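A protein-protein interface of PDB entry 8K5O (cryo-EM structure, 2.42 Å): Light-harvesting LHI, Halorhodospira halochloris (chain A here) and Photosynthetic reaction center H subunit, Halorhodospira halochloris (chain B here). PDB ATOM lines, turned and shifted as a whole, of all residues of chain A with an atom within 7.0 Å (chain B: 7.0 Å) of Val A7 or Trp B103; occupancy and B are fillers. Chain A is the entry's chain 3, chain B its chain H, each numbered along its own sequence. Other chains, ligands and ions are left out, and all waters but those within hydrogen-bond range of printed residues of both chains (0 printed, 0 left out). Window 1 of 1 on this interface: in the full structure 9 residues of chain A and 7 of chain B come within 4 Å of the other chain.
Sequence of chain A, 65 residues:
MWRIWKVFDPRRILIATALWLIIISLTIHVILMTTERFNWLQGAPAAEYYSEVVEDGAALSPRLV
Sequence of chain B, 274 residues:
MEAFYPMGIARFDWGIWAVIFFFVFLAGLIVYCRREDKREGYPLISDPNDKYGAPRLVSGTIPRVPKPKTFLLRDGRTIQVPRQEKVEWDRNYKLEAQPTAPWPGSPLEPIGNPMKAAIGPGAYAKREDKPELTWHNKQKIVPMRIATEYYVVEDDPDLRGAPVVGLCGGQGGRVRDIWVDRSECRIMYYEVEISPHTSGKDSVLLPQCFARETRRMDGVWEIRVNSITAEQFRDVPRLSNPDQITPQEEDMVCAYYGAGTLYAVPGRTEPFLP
O of Pro B104 lies close to NH1 of Arg A12. NE1 of Trp B103 is in hydrogen-bond range of O of Phe A8, at 3.1 Å. The indole nitrogen (NE1) of Trp B103 lies within hydrogen-bond range of the backbone carbonyl oxygen (O) of Trp A5 (2.5 Å). The indole nitrogen (NE1) of Trp B103 sits close to the backbone carbonyl oxygen (O) of Lys A6 (3.5 Å). The guanidinium group (NH2) of Arg A12 lies within hydrogen-bond range of the side-chain hydroxyl (OG) of Ser B106, 2.4 Å away.
OG of Ser B106 is in hydrogen-bond range of O of Ala B101 (3.2 Å). ND2 of Asn B49 sits at hydrogen-bond distance from O of Ala B101 (2.4 Å). The side-chain carboxylate (OD1) of Asp B50 sits close to the backbone NH (N) of Tyr B52. The side-chain carboxylate of Asp B47 is in hydrogen-bond range of the backbone NH of Gly B105. NE of Arg A12 is in salt-bridge range of OD2 of Asp A9. OG of Ser B106 sits at hydrogen-bond distance from O of Trp B103 (2.5 Å).
Tyr B52 touches Arg A3 (OH to O, 3.5 Å). Lys A6 touches Lys B51 (CB to CD, 3.6 Å). Tyr B52 touches Lys A6 (CE1 to CB, 3.7 Å). Tyr B52 touches Val A7 (CE1 to CG2, 3.4 Å). Trp B103 touches Val A7. Trp B103 touches Asp A9 (CZ3 to OD1, 3.1 Å). Trp B103 touches Pro A10 (CZ2 to CD, 3.3 Å). Arg A11 touches Ala B101 (NH2 to CB, 3.2 Å). Trp B103 touches Arg A12. Arg A12 touches Gly B105.
Of chain B, only Tyr B52 and Trp B103 come within 4 Å of Val A7. Of the printed residues of chain B, Phe A8 touches Trp B103 (3.1 Å). Of the printed residues of chain B, Asp A9 touches Trp B103. Of the printed residues of chain A, Lys B51 touches Lys A6. Of the printed residues of chain A, Ala B101 touches Arg A11 (3.2 Å). Of chain A, only Trp A5 (2.5 Å), Lys A6 (3.3 Å), Val A7 (3.5 Å), Phe A8 (3.1 Å), Asp A9 (3.1 Å), Pro A10 (3.3 Å), Arg A11 (3.9 Å) and Arg A12 (3.6 Å) come within 4 Å of Trp B103. The nearest residue of chain A that does not touch Trp B103 is Ile A4 (5.3 Å). The nearest printed residue of chain B that does not touch Arg A12 is Ala B101 (4.3 Å).
Of the 11 printed residues of chain A, 9 touch a printed residue of chain B. Printed residues of chain A that touch a printed residue of chain B: Arg A3, Trp A5, Lys A6, Val A7, Phe A8, Asp A9, Pro A10, Arg A11 and Arg A12. Hydrophobic or aromatic side chains of chain A that line the printed part of chain B: Val A7 and Pro A10. Printed residues of chain B that touch a printed residue of chain A: Lys B51, Tyr B52, Ala B101, Trp B103, Pro B104, Gly B105 and Ser B106. Hydrophobic or aromatic side chains of chain B within 4 Å of the printed part of chain A: Tyr B52, Ala B101 and Trp B103. Among the printed residues, no Asp or Glu carboxylate lies within 4 Å of a Lys or Arg side-chain nitrogen of the other chain.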
ATOM      1  N   TRP A   2       2.139 -32.084  -0.455  1.00  0.00           N
ATOM      2  CA  TRP A   2       3.016 -31.118  -1.110  1.00  0.00           C
ATOM      3  C   TRP A   2       2.401 -29.725  -1.109  1.00  0.00           C
ATOM      4  O   TRP A   2       3.126 -28.723  -1.092  1.00  0.00           O
ATOM      5  CB  TRP A   2       3.334 -31.566  -2.537  1.00  0.00           C
ATOM      6  CG  TRP A   2       2.155 -31.660  -3.445  1.00  0.00           C
ATOM      7  CD1 TRP A   2       1.403 -32.764  -3.701  1.00  0.00           C
ATOM      8  CD2 TRP A   2       1.596 -30.602  -4.228  1.00  0.00           C
ATOM      9  NE1 TRP A   2       0.408 -32.462  -4.595  1.00  0.00           N
ATOM     10  CE2 TRP A   2       0.506 -31.140  -4.935  1.00  0.00           C
ATOM     11  CE3 TRP A   2       1.915 -29.254  -4.406  1.00  0.00           C
ATOM     12  CZ2 TRP A   2      -0.268 -30.376  -5.801  1.00  0.00           C
ATOM     13  CZ3 TRP A   2       1.144 -28.499  -5.259  1.00  0.00           C
ATOM     14  CH2 TRP A   2       0.065 -29.060  -5.947  1.00  0.00           C
ATOM     15  N   ARG A   3       1.070 -29.645  -1.083  1.00  0.00           N
ATOM     16  CA  ARG A   3       0.388 -28.359  -1.127  1.00  0.00           C
ATOM     17  C   ARG A   3       0.639 -27.532   0.123  1.00  0.00           C
ATOM     18  O   ARG A   3       0.290 -26.348   0.146  1.00  0.00           O
ATOM     19  CB  ARG A   3      -1.111 -28.572  -1.327  1.00  0.00           C
ATOM     20  CG  ARG A   3      -1.456 -29.263  -2.629  1.00  0.00           C
ATOM     21  CD  ARG A   3      -2.947 -29.496  -2.759  1.00  0.00           C
ATOM     22  NE  ARG A   3      -3.266 -30.318  -3.919  1.00  0.00           N
ATOM     23  CZ  ARG A   3      -3.500 -29.842  -5.134  1.00  0.00           C
ATOM     24  NH1 ARG A   3      -3.456 -28.545  -5.389  1.00  0.00           N
ATOM     25  NH2 ARG A   3      -3.782 -30.690  -6.119  1.00  0.00           N
ATOM     26  N   ILE A   4       1.215 -28.130   1.169  1.00  0.00           N
ATOM     27  CA  ILE A   4       1.609 -27.362   2.342  1.00  0.00           C
ATOM     28  C   ILE A   4       2.655 -26.328   1.977  1.00  0.00           C
ATOM     29  O   ILE A   4       2.786 -25.310   2.663  1.00  0.00           O
ATOM     30  CB  ILE A   4       2.107 -28.294   3.470  1.00  0.00           C
ATOM     31  CG1 ILE A   4       2.044 -27.579   4.819  1.00  0.00           C
ATOM     32  CG2 ILE A   4       3.525 -28.761   3.206  1.00  0.00           C
ATOM     33  CD1 ILE A   4       0.651 -27.224   5.246  1.00  0.00           C
ATOM     34  N   TRP A   5       3.396 -26.555   0.895  1.00  0.00           N
ATOM     35  CA  TRP A   5       4.359 -25.568   0.438  1.00  0.00           C
ATOM     36  C   TRP A   5       3.699 -24.414  -0.293  1.00  0.00           C
ATOM     37  O   TRP A   5       4.353 -23.394  -0.525  1.00  0.00           O
ATOM     38  CB  TRP A   5       5.408 -26.249  -0.432  1.00  0.00           C
ATOM     39  CG  TRP A   5       5.990 -27.424   0.269  1.00  0.00           C
ATOM     40  CD1 TRP A   5       6.047 -28.701  -0.191  1.00  0.00           C
ATOM     41  CD2 TRP A   5       6.568 -27.442   1.579  1.00  0.00           C
ATOM     42  NE1 TRP A   5       6.635 -29.512   0.742  1.00  0.00           N
ATOM     43  CE2 TRP A   5       6.964 -28.763   1.839  1.00  0.00           C
ATOM     44  CE3 TRP A   5       6.797 -26.467   2.554  1.00  0.00           C
ATOM     45  CZ2 TRP A   5       7.579 -29.135   3.028  1.00  0.00           C
ATOM     46  CZ3 TRP A   5       7.400 -26.838   3.731  1.00  0.00           C
ATOM     47  CH2 TRP A   5       7.785 -28.160   3.960  1.00  0.00           C
ATOM     48  N   LYS A   6       2.427 -24.553  -0.657  1.00  0.00           N
ATOM     49  CA  LYS A   6       1.620 -23.391  -0.986  1.00  0.00           C
ATOM     50  C   LYS A   6       1.210 -22.635   0.268  1.00  0.00           C
ATOM     51  O   LYS A   6       1.050 -21.411   0.226  1.00  0.00           O
ATOM     52  CB  LYS A   6       0.382 -23.812  -1.776  1.00  0.00           C
ATOM     53  CG  LYS A   6       0.689 -24.543  -3.064  1.00  0.00           C
ATOM     54  CD  LYS A   6      -0.503 -25.348  -3.537  1.00  0.00           C
ATOM     55  CE  LYS A   6      -1.615 -24.441  -4.022  1.00  0.00           C
ATOM     56  NZ  LYS A   6      -2.430 -25.091  -5.082  1.00  0.00           N
ATOM     57  N   VAL A   7       1.039 -23.342   1.384  1.00  0.00           N
ATOM     58  CA  VAL A   7       0.668 -22.694   2.636  1.00  0.00           C
ATOM     59  C   VAL A   7       1.876 -22.027   3.273  1.00  0.00           C
ATOM     60  O   VAL A   7       1.838 -20.847   3.635  1.00  0.00           O
ATOM     61  CB  VAL A   7       0.028 -23.712   3.598  1.00  0.00           C
ATOM     62  CG1 VAL A   7      -0.504 -23.008   4.822  1.00  0.00           C
ATOM     63  CG2 VAL A   7      -1.067 -24.485   2.906  1.00  0.00           C
ATOM     64  N   PHE A   8       2.960 -22.773   3.424  1.00  0.00           N
ATOM     65  CA  PHE A   8       4.139 -22.311   4.132  1.00  0.00           C
ATOM     66  C   PHE A   8       5.319 -22.248   3.180  1.00  0.00           C
ATOM     67  O   PHE A   8       5.418 -23.031   2.234  1.00  0.00           O
ATOM     68  CB  PHE A   8       4.480 -23.230   5.304  1.00  0.00           C
ATOM     69  CG  PHE A   8       3.458 -23.223   6.394  1.00  0.00           C
ATOM     70  CD1 PHE A   8       3.430 -22.204   7.326  1.00  0.00           C
ATOM     71  CD2 PHE A   8       2.526 -24.237   6.489  1.00  0.00           C
ATOM     72  CE1 PHE A   8       2.491 -22.197   8.326  1.00  0.00           C
ATOM     73  CE2 PHE A   8       1.587 -24.230   7.488  1.00  0.00           C
ATOM     74  CZ  PHE A   8       1.571 -23.212   8.408  1.00  0.00           C
ATOM     75  N   ASP A   9       6.206 -21.308   3.442  1.00  0.00           N
ATOM     76  CA  ASP A   9       7.442 -21.210   2.690  1.00  0.00           C
ATOM     77  C   ASP A   9       8.304 -22.426   2.994  1.00  0.00           C
ATOM     78  O   ASP A   9       8.603 -22.682   4.167  1.00  0.00           O
ATOM     79  CB  ASP A   9       8.169 -19.925   3.061  1.00  0.00           C
ATOM     80  CG  ASP A   9       9.337 -19.624   2.153  1.00  0.00           C
ATOM     81  OD1 ASP A   9       9.640 -20.436   1.259  1.00  0.00           O
ATOM     82  OD2 ASP A   9       9.959 -18.560   2.332  1.00  0.00           O
ATOM     83  N   PRO A  10       8.702 -23.208   1.991  1.00  0.00           N
ATOM     84  CA  PRO A  10       9.636 -24.308   2.259  1.00  0.00           C
ATOM     85  C   PRO A  10      10.913 -23.846   2.922  1.00  0.00           C
ATOM     86  O   PRO A  10      11.468 -24.564   3.756  1.00  0.00           O
ATOM     87  CB  PRO A  10       9.890 -24.873   0.858  1.00  0.00           C
ATOM     88  CG  PRO A  10       8.663 -24.582   0.122  1.00  0.00           C
ATOM     89  CD  PRO A  10       8.211 -23.245   0.609  1.00  0.00           C
ATOM     90  N   ARG A  11      11.398 -22.658   2.565  1.00  0.00           N
ATOM     91  CA  ARG A  11      12.589 -22.107   3.198  1.00  0.00           C
ATOM     92  C   ARG A  11      12.359 -21.823   4.676  1.00  0.00           C
ATOM     93  O   ARG A  11      13.219 -22.121   5.510  1.00  0.00           O
ATOM     94  CB  ARG A  11      13.008 -20.843   2.457  1.00  0.00           C
ATOM     95  CG  ARG A  11      13.692 -21.134   1.149  1.00  0.00           C
ATOM     96  CD  ARG A  11      14.077 -19.868   0.431  1.00  0.00           C
ATOM     97  NE  ARG A  11      12.903 -19.197  -0.110  1.00  0.00           N
ATOM     98  CZ  ARG A  11      12.464 -18.013   0.288  1.00  0.00           C
ATOM     99  NH1 ARG A  11      13.089 -17.326   1.230  1.00  0.00           N
ATOM    100  NH2 ARG A  11      11.372 -17.506  -0.272  1.00  0.00           N
ATOM    101  N   ARG A  12      11.205 -21.254   5.022  1.00  0.00           N
ATOM    102  CA  ARG A  12      10.928 -20.948   6.421  1.00  0.00           C
ATOM    103  C   ARG A  12      10.711 -22.213   7.235  1.00  0.00           C
ATOM    104  O   ARG A  12      11.159 -22.301   8.381  1.00  0.00           O
ATOM    105  CB  ARG A  12       9.716 -20.030   6.523  1.00  0.00           C
ATOM    106  CG  ARG A  12       9.948 -18.686   5.901  1.00  0.00           C
ATOM    107  CD  ARG A  12       8.703 -17.849   5.915  1.00  0.00           C
ATOM    108  NE  ARG A  12       8.612 -17.036   4.714  1.00  0.00           N
ATOM    109  CZ  ARG A  12       7.576 -16.271   4.412  1.00  0.00           C
ATOM    110  NH1 ARG A  12       6.532 -16.178   5.217  1.00  0.00           N
ATOM    111  NH2 ARG A  12       7.588 -15.584   3.275  1.00  0.00           N
ATOM    112  N   ASP B  47      -2.103 -11.244   5.182  1.00  0.00           N
ATOM    113  CA  ASP B  47      -1.188 -10.855   4.121  1.00  0.00           C
ATOM    114  C   ASP B  47      -1.822 -11.147   2.767  1.00  0.00           C
ATOM    115  O   ASP B  47      -2.162 -12.305   2.490  1.00  0.00           O
ATOM    116  CB  ASP B  47       0.139 -11.601   4.255  1.00  0.00           C
ATOM    117  CG  ASP B  47       1.266 -10.945   3.477  1.00  0.00           C
ATOM    118  OD1 ASP B  47       1.008 -10.385   2.395  1.00  0.00           O
ATOM    119  OD2 ASP B  47       2.422 -10.998   3.946  1.00  0.00           O
ATOM    120  N   ASN B  49      -0.313 -11.332   0.023  1.00  0.00           N
ATOM    121  CA  ASN B  49       0.593 -12.276  -0.610  1.00  0.00           C
ATOM    122  C   ASN B  49       0.364 -13.656  -0.012  1.00  0.00           C
ATOM    123  O   ASN B  49       0.949 -14.006   1.015  1.00  0.00           O
ATOM    124  CB  ASN B  49       2.041 -11.835  -0.432  1.00  0.00           C
ATOM    125  CG  ASN B  49       3.008 -12.736  -1.149  1.00  0.00           C
ATOM    126  OD1 ASN B  49       2.762 -13.152  -2.278  1.00  0.00           O
ATOM    127  ND2 ASN B  49       4.119 -13.044  -0.500  1.00  0.00           N
ATOM    128  N   ASP B  50      -0.499 -14.436  -0.652  1.00  0.00           N
ATOM    129  CA  ASP B  50      -0.949 -15.705  -0.101  1.00  0.00           C
ATOM    130  C   ASP B  50      -1.622 -16.487  -1.213  1.00  0.00           C
ATOM    131  O   ASP B  50      -2.498 -15.955  -1.899  1.00  0.00           O
ATOM    132  CB  ASP B  50      -1.920 -15.477   1.064  1.00  0.00           C
ATOM    133  CG  ASP B  50      -2.245 -16.746   1.817  1.00  0.00           C
ATOM    134  OD1 ASP B  50      -1.679 -17.804   1.480  1.00  0.00           O
ATOM    135  OD2 ASP B  50      -3.069 -16.684   2.751  1.00  0.00           O
ATOM    136  N   LYS B  51      -1.212 -17.741  -1.390  1.00  0.00           N
ATOM    137  CA  LYS B  51      -1.851 -18.584  -2.389  1.00  0.00           C
ATOM    138  C   LYS B  51      -3.262 -18.987  -1.990  1.00  0.00           C
ATOM    139  O   LYS B  51      -4.002 -19.503  -2.832  1.00  0.00           O
ATOM    140  CB  LYS B  51      -1.012 -19.832  -2.646  1.00  0.00           C
ATOM    141  CG  LYS B  51       0.386 -19.533  -3.144  1.00  0.00           C
ATOM    142  CD  LYS B  51       1.099 -20.802  -3.531  1.00  0.00           C
ATOM    143  CE  LYS B  51       2.523 -20.534  -3.953  1.00  0.00           C
ATOM    144  NZ  LYS B  51       3.359 -20.154  -2.787  1.00  0.00           N
ATOM    145  N   TYR B  52      -3.649 -18.759  -0.740  1.00  0.00           N
ATOM    146  CA  TYR B  52      -4.976 -19.086  -0.252  1.00  0.00           C
ATOM    147  C   TYR B  52      -5.725 -17.815   0.121  1.00  0.00           C
ATOM    148  O   TYR B  52      -5.131 -16.758   0.347  1.00  0.00           O
ATOM    149  CB  TYR B  52      -4.901 -20.035   0.948  1.00  0.00           C
ATOM    150  CG  TYR B  52      -4.385 -21.403   0.581  1.00  0.00           C
ATOM    151  CD1 TYR B  52      -3.028 -21.686   0.606  1.00  0.00           C
ATOM    152  CD2 TYR B  52      -5.256 -22.409   0.197  1.00  0.00           C
ATOM    153  CE1 TYR B  52      -2.556 -22.931   0.260  1.00  0.00           C
ATOM    154  CE2 TYR B  52      -4.795 -23.658  -0.146  1.00  0.00           C
ATOM    155  CZ  TYR B  52      -3.445 -23.916  -0.110  1.00  0.00           C
ATOM    156  OH  TYR B  52      -2.985 -25.163  -0.453  1.00  0.00           O
ATOM    157  N   PRO B  99       6.272  -8.700  -3.243  1.00  0.00           N
ATOM    158  CA  PRO B  99       6.777  -9.652  -2.251  1.00  0.00           C
ATOM    159  C   PRO B  99       7.946 -10.440  -2.821  1.00  0.00           C
ATOM    160  O   PRO B  99       7.980 -10.763  -4.008  1.00  0.00           O
ATOM    161  CB  PRO B  99       5.569 -10.549  -1.971  1.00  0.00           C
ATOM    162  CG  PRO B  99       4.388  -9.795  -2.484  1.00  0.00           C
ATOM    163  CD  PRO B  99       4.882  -8.987  -3.627  1.00  0.00           C
ATOM    164  N   THR B 100       8.923 -10.733  -1.966  1.00  0.00           N
ATOM    165  CA  THR B 100      10.061 -11.521  -2.421  1.00  0.00           C
ATOM    166  C   THR B 100       9.662 -12.963  -2.695  1.00  0.00           C
ATOM    167  O   THR B 100      10.223 -13.601  -3.592  1.00  0.00           O
ATOM    168  CB  THR B 100      11.189 -11.464  -1.394  1.00  0.00           C
ATOM    169  OG1 THR B 100      10.737 -12.021  -0.155  1.00  0.00           O
ATOM    170  CG2 THR B 100      11.623 -10.028  -1.169  1.00  0.00           C
ATOM    171  N   ALA B 101       8.703 -13.481  -1.946  1.00  0.00           N
ATOM    172  CA  ALA B 101       8.229 -14.851  -2.030  1.00  0.00           C
ATOM    173  C   ALA B 101       6.709 -14.850  -2.040  1.00  0.00           C
ATOM    174  O   ALA B 101       6.082 -13.870  -1.626  1.00  0.00           O
ATOM    175  CB  ALA B 101       8.750 -15.681  -0.849  1.00  0.00           C
ATOM    176  N   PRO B 102       6.085 -15.924  -2.527  1.00  0.00           N
ATOM    177  CA  PRO B 102       4.620 -15.975  -2.598  1.00  0.00           C
ATOM    178  C   PRO B 102       3.918 -16.350  -1.301  1.00  0.00           C
ATOM    179  O   PRO B 102       2.738 -16.705  -1.347  1.00  0.00           O
ATOM    180  CB  PRO B 102       4.378 -17.049  -3.670  1.00  0.00           C
ATOM    181  CG  PRO B 102       5.565 -17.913  -3.598  1.00  0.00           C
ATOM    182  CD  PRO B 102       6.709 -17.013  -3.298  1.00  0.00           C
ATOM    183  N   TRP B 103       4.581 -16.289  -0.153  1.00  0.00           N
ATOM    184  CA  TRP B 103       3.921 -16.693   1.078  1.00  0.00           C
ATOM    185  C   TRP B 103       3.722 -15.503   2.008  1.00  0.00           C
ATOM    186  O   TRP B 103       4.457 -14.515   1.928  1.00  0.00           O
ATOM    187  CB  TRP B 103       4.726 -17.771   1.815  1.00  0.00           C
ATOM    188  CG  TRP B 103       4.881 -19.003   1.019  1.00  0.00           C
ATOM    189  CD1 TRP B 103       4.014 -20.046   0.947  1.00  0.00           C
ATOM    190  CD2 TRP B 103       5.965 -19.318   0.149  1.00  0.00           C
ATOM    191  NE1 TRP B 103       4.495 -21.001   0.093  1.00  0.00           N
ATOM    192  CE2 TRP B 103       5.696 -20.577  -0.410  1.00  0.00           C
ATOM    193  CE3 TRP B 103       7.142 -18.660  -0.207  1.00  0.00           C
ATOM    194  CZ2 TRP B 103       6.555 -21.184  -1.309  1.00  0.00           C
ATOM    195  CZ3 TRP B 103       7.995 -19.269  -1.093  1.00  0.00           C
ATOM    196  CH2 TRP B 103       7.702 -20.519  -1.631  1.00  0.00           C
ATOM    197  N   PRO B 104       2.733 -15.565   2.896  1.00  0.00           N
ATOM    198  CA  PRO B 104       2.570 -14.501   3.888  1.00  0.00           C
ATOM    199  C   PRO B 104       3.795 -14.396   4.780  1.00  0.00           C
ATOM    200  O   PRO B 104       4.462 -15.387   5.082  1.00  0.00           O
ATOM    201  CB  PRO B 104       1.338 -14.942   4.681  1.00  0.00           C
ATOM    202  CG  PRO B 104       0.624 -15.871   3.793  1.00  0.00           C
ATOM    203  CD  PRO B 104       1.663 -16.570   2.992  1.00  0.00           C
ATOM    204  N   GLY B 105       4.085 -13.175   5.206  1.00  0.00           N
ATOM    205  CA  GLY B 105       5.298 -12.895   5.932  1.00  0.00           C
ATOM    206  C   GLY B 105       6.490 -12.600   5.060  1.00  0.00           C
ATOM    207  O   GLY B 105       7.572 -12.324   5.589  1.00  0.00           O
ATOM    208  N   SER B 106       6.329 -12.654   3.745  1.00  0.00           N
ATOM    209  CA  SER B 106       7.420 -12.324   2.849  1.00  0.00           C
ATOM    210  C   SER B 106       7.650 -10.817   2.846  1.00  0.00           C
ATOM    211  O   SER B 106       6.690 -10.040   2.832  1.00  0.00           O
ATOM    212  CB  SER B 106       7.113 -12.802   1.435  1.00  0.00           C
ATOM    213  OG  SER B 106       6.923 -14.202   1.408  1.00  0.00           O
ATOM    214  N   PRO B 107       8.900 -10.372   2.864  1.00  0.00           N
ATOM    215  CA  PRO B 107       9.171  -8.939   2.761  1.00  0.00           C
ATOM    216  C   PRO B 107       8.886  -8.427   1.359  1.00  0.00           C
ATOM    217  O   PRO B 107       8.779  -9.187   0.394  1.00  0.00           O
ATOM    218  CB  PRO B 107      10.659  -8.841   3.101  1.00  0.00           C
ATOM    219  CG  PRO B 107      11.208 -10.151   2.694  1.00  0.00           C
ATOM    220  CD  PRO B 107      10.137 -11.160   2.985  1.00  0.00           C
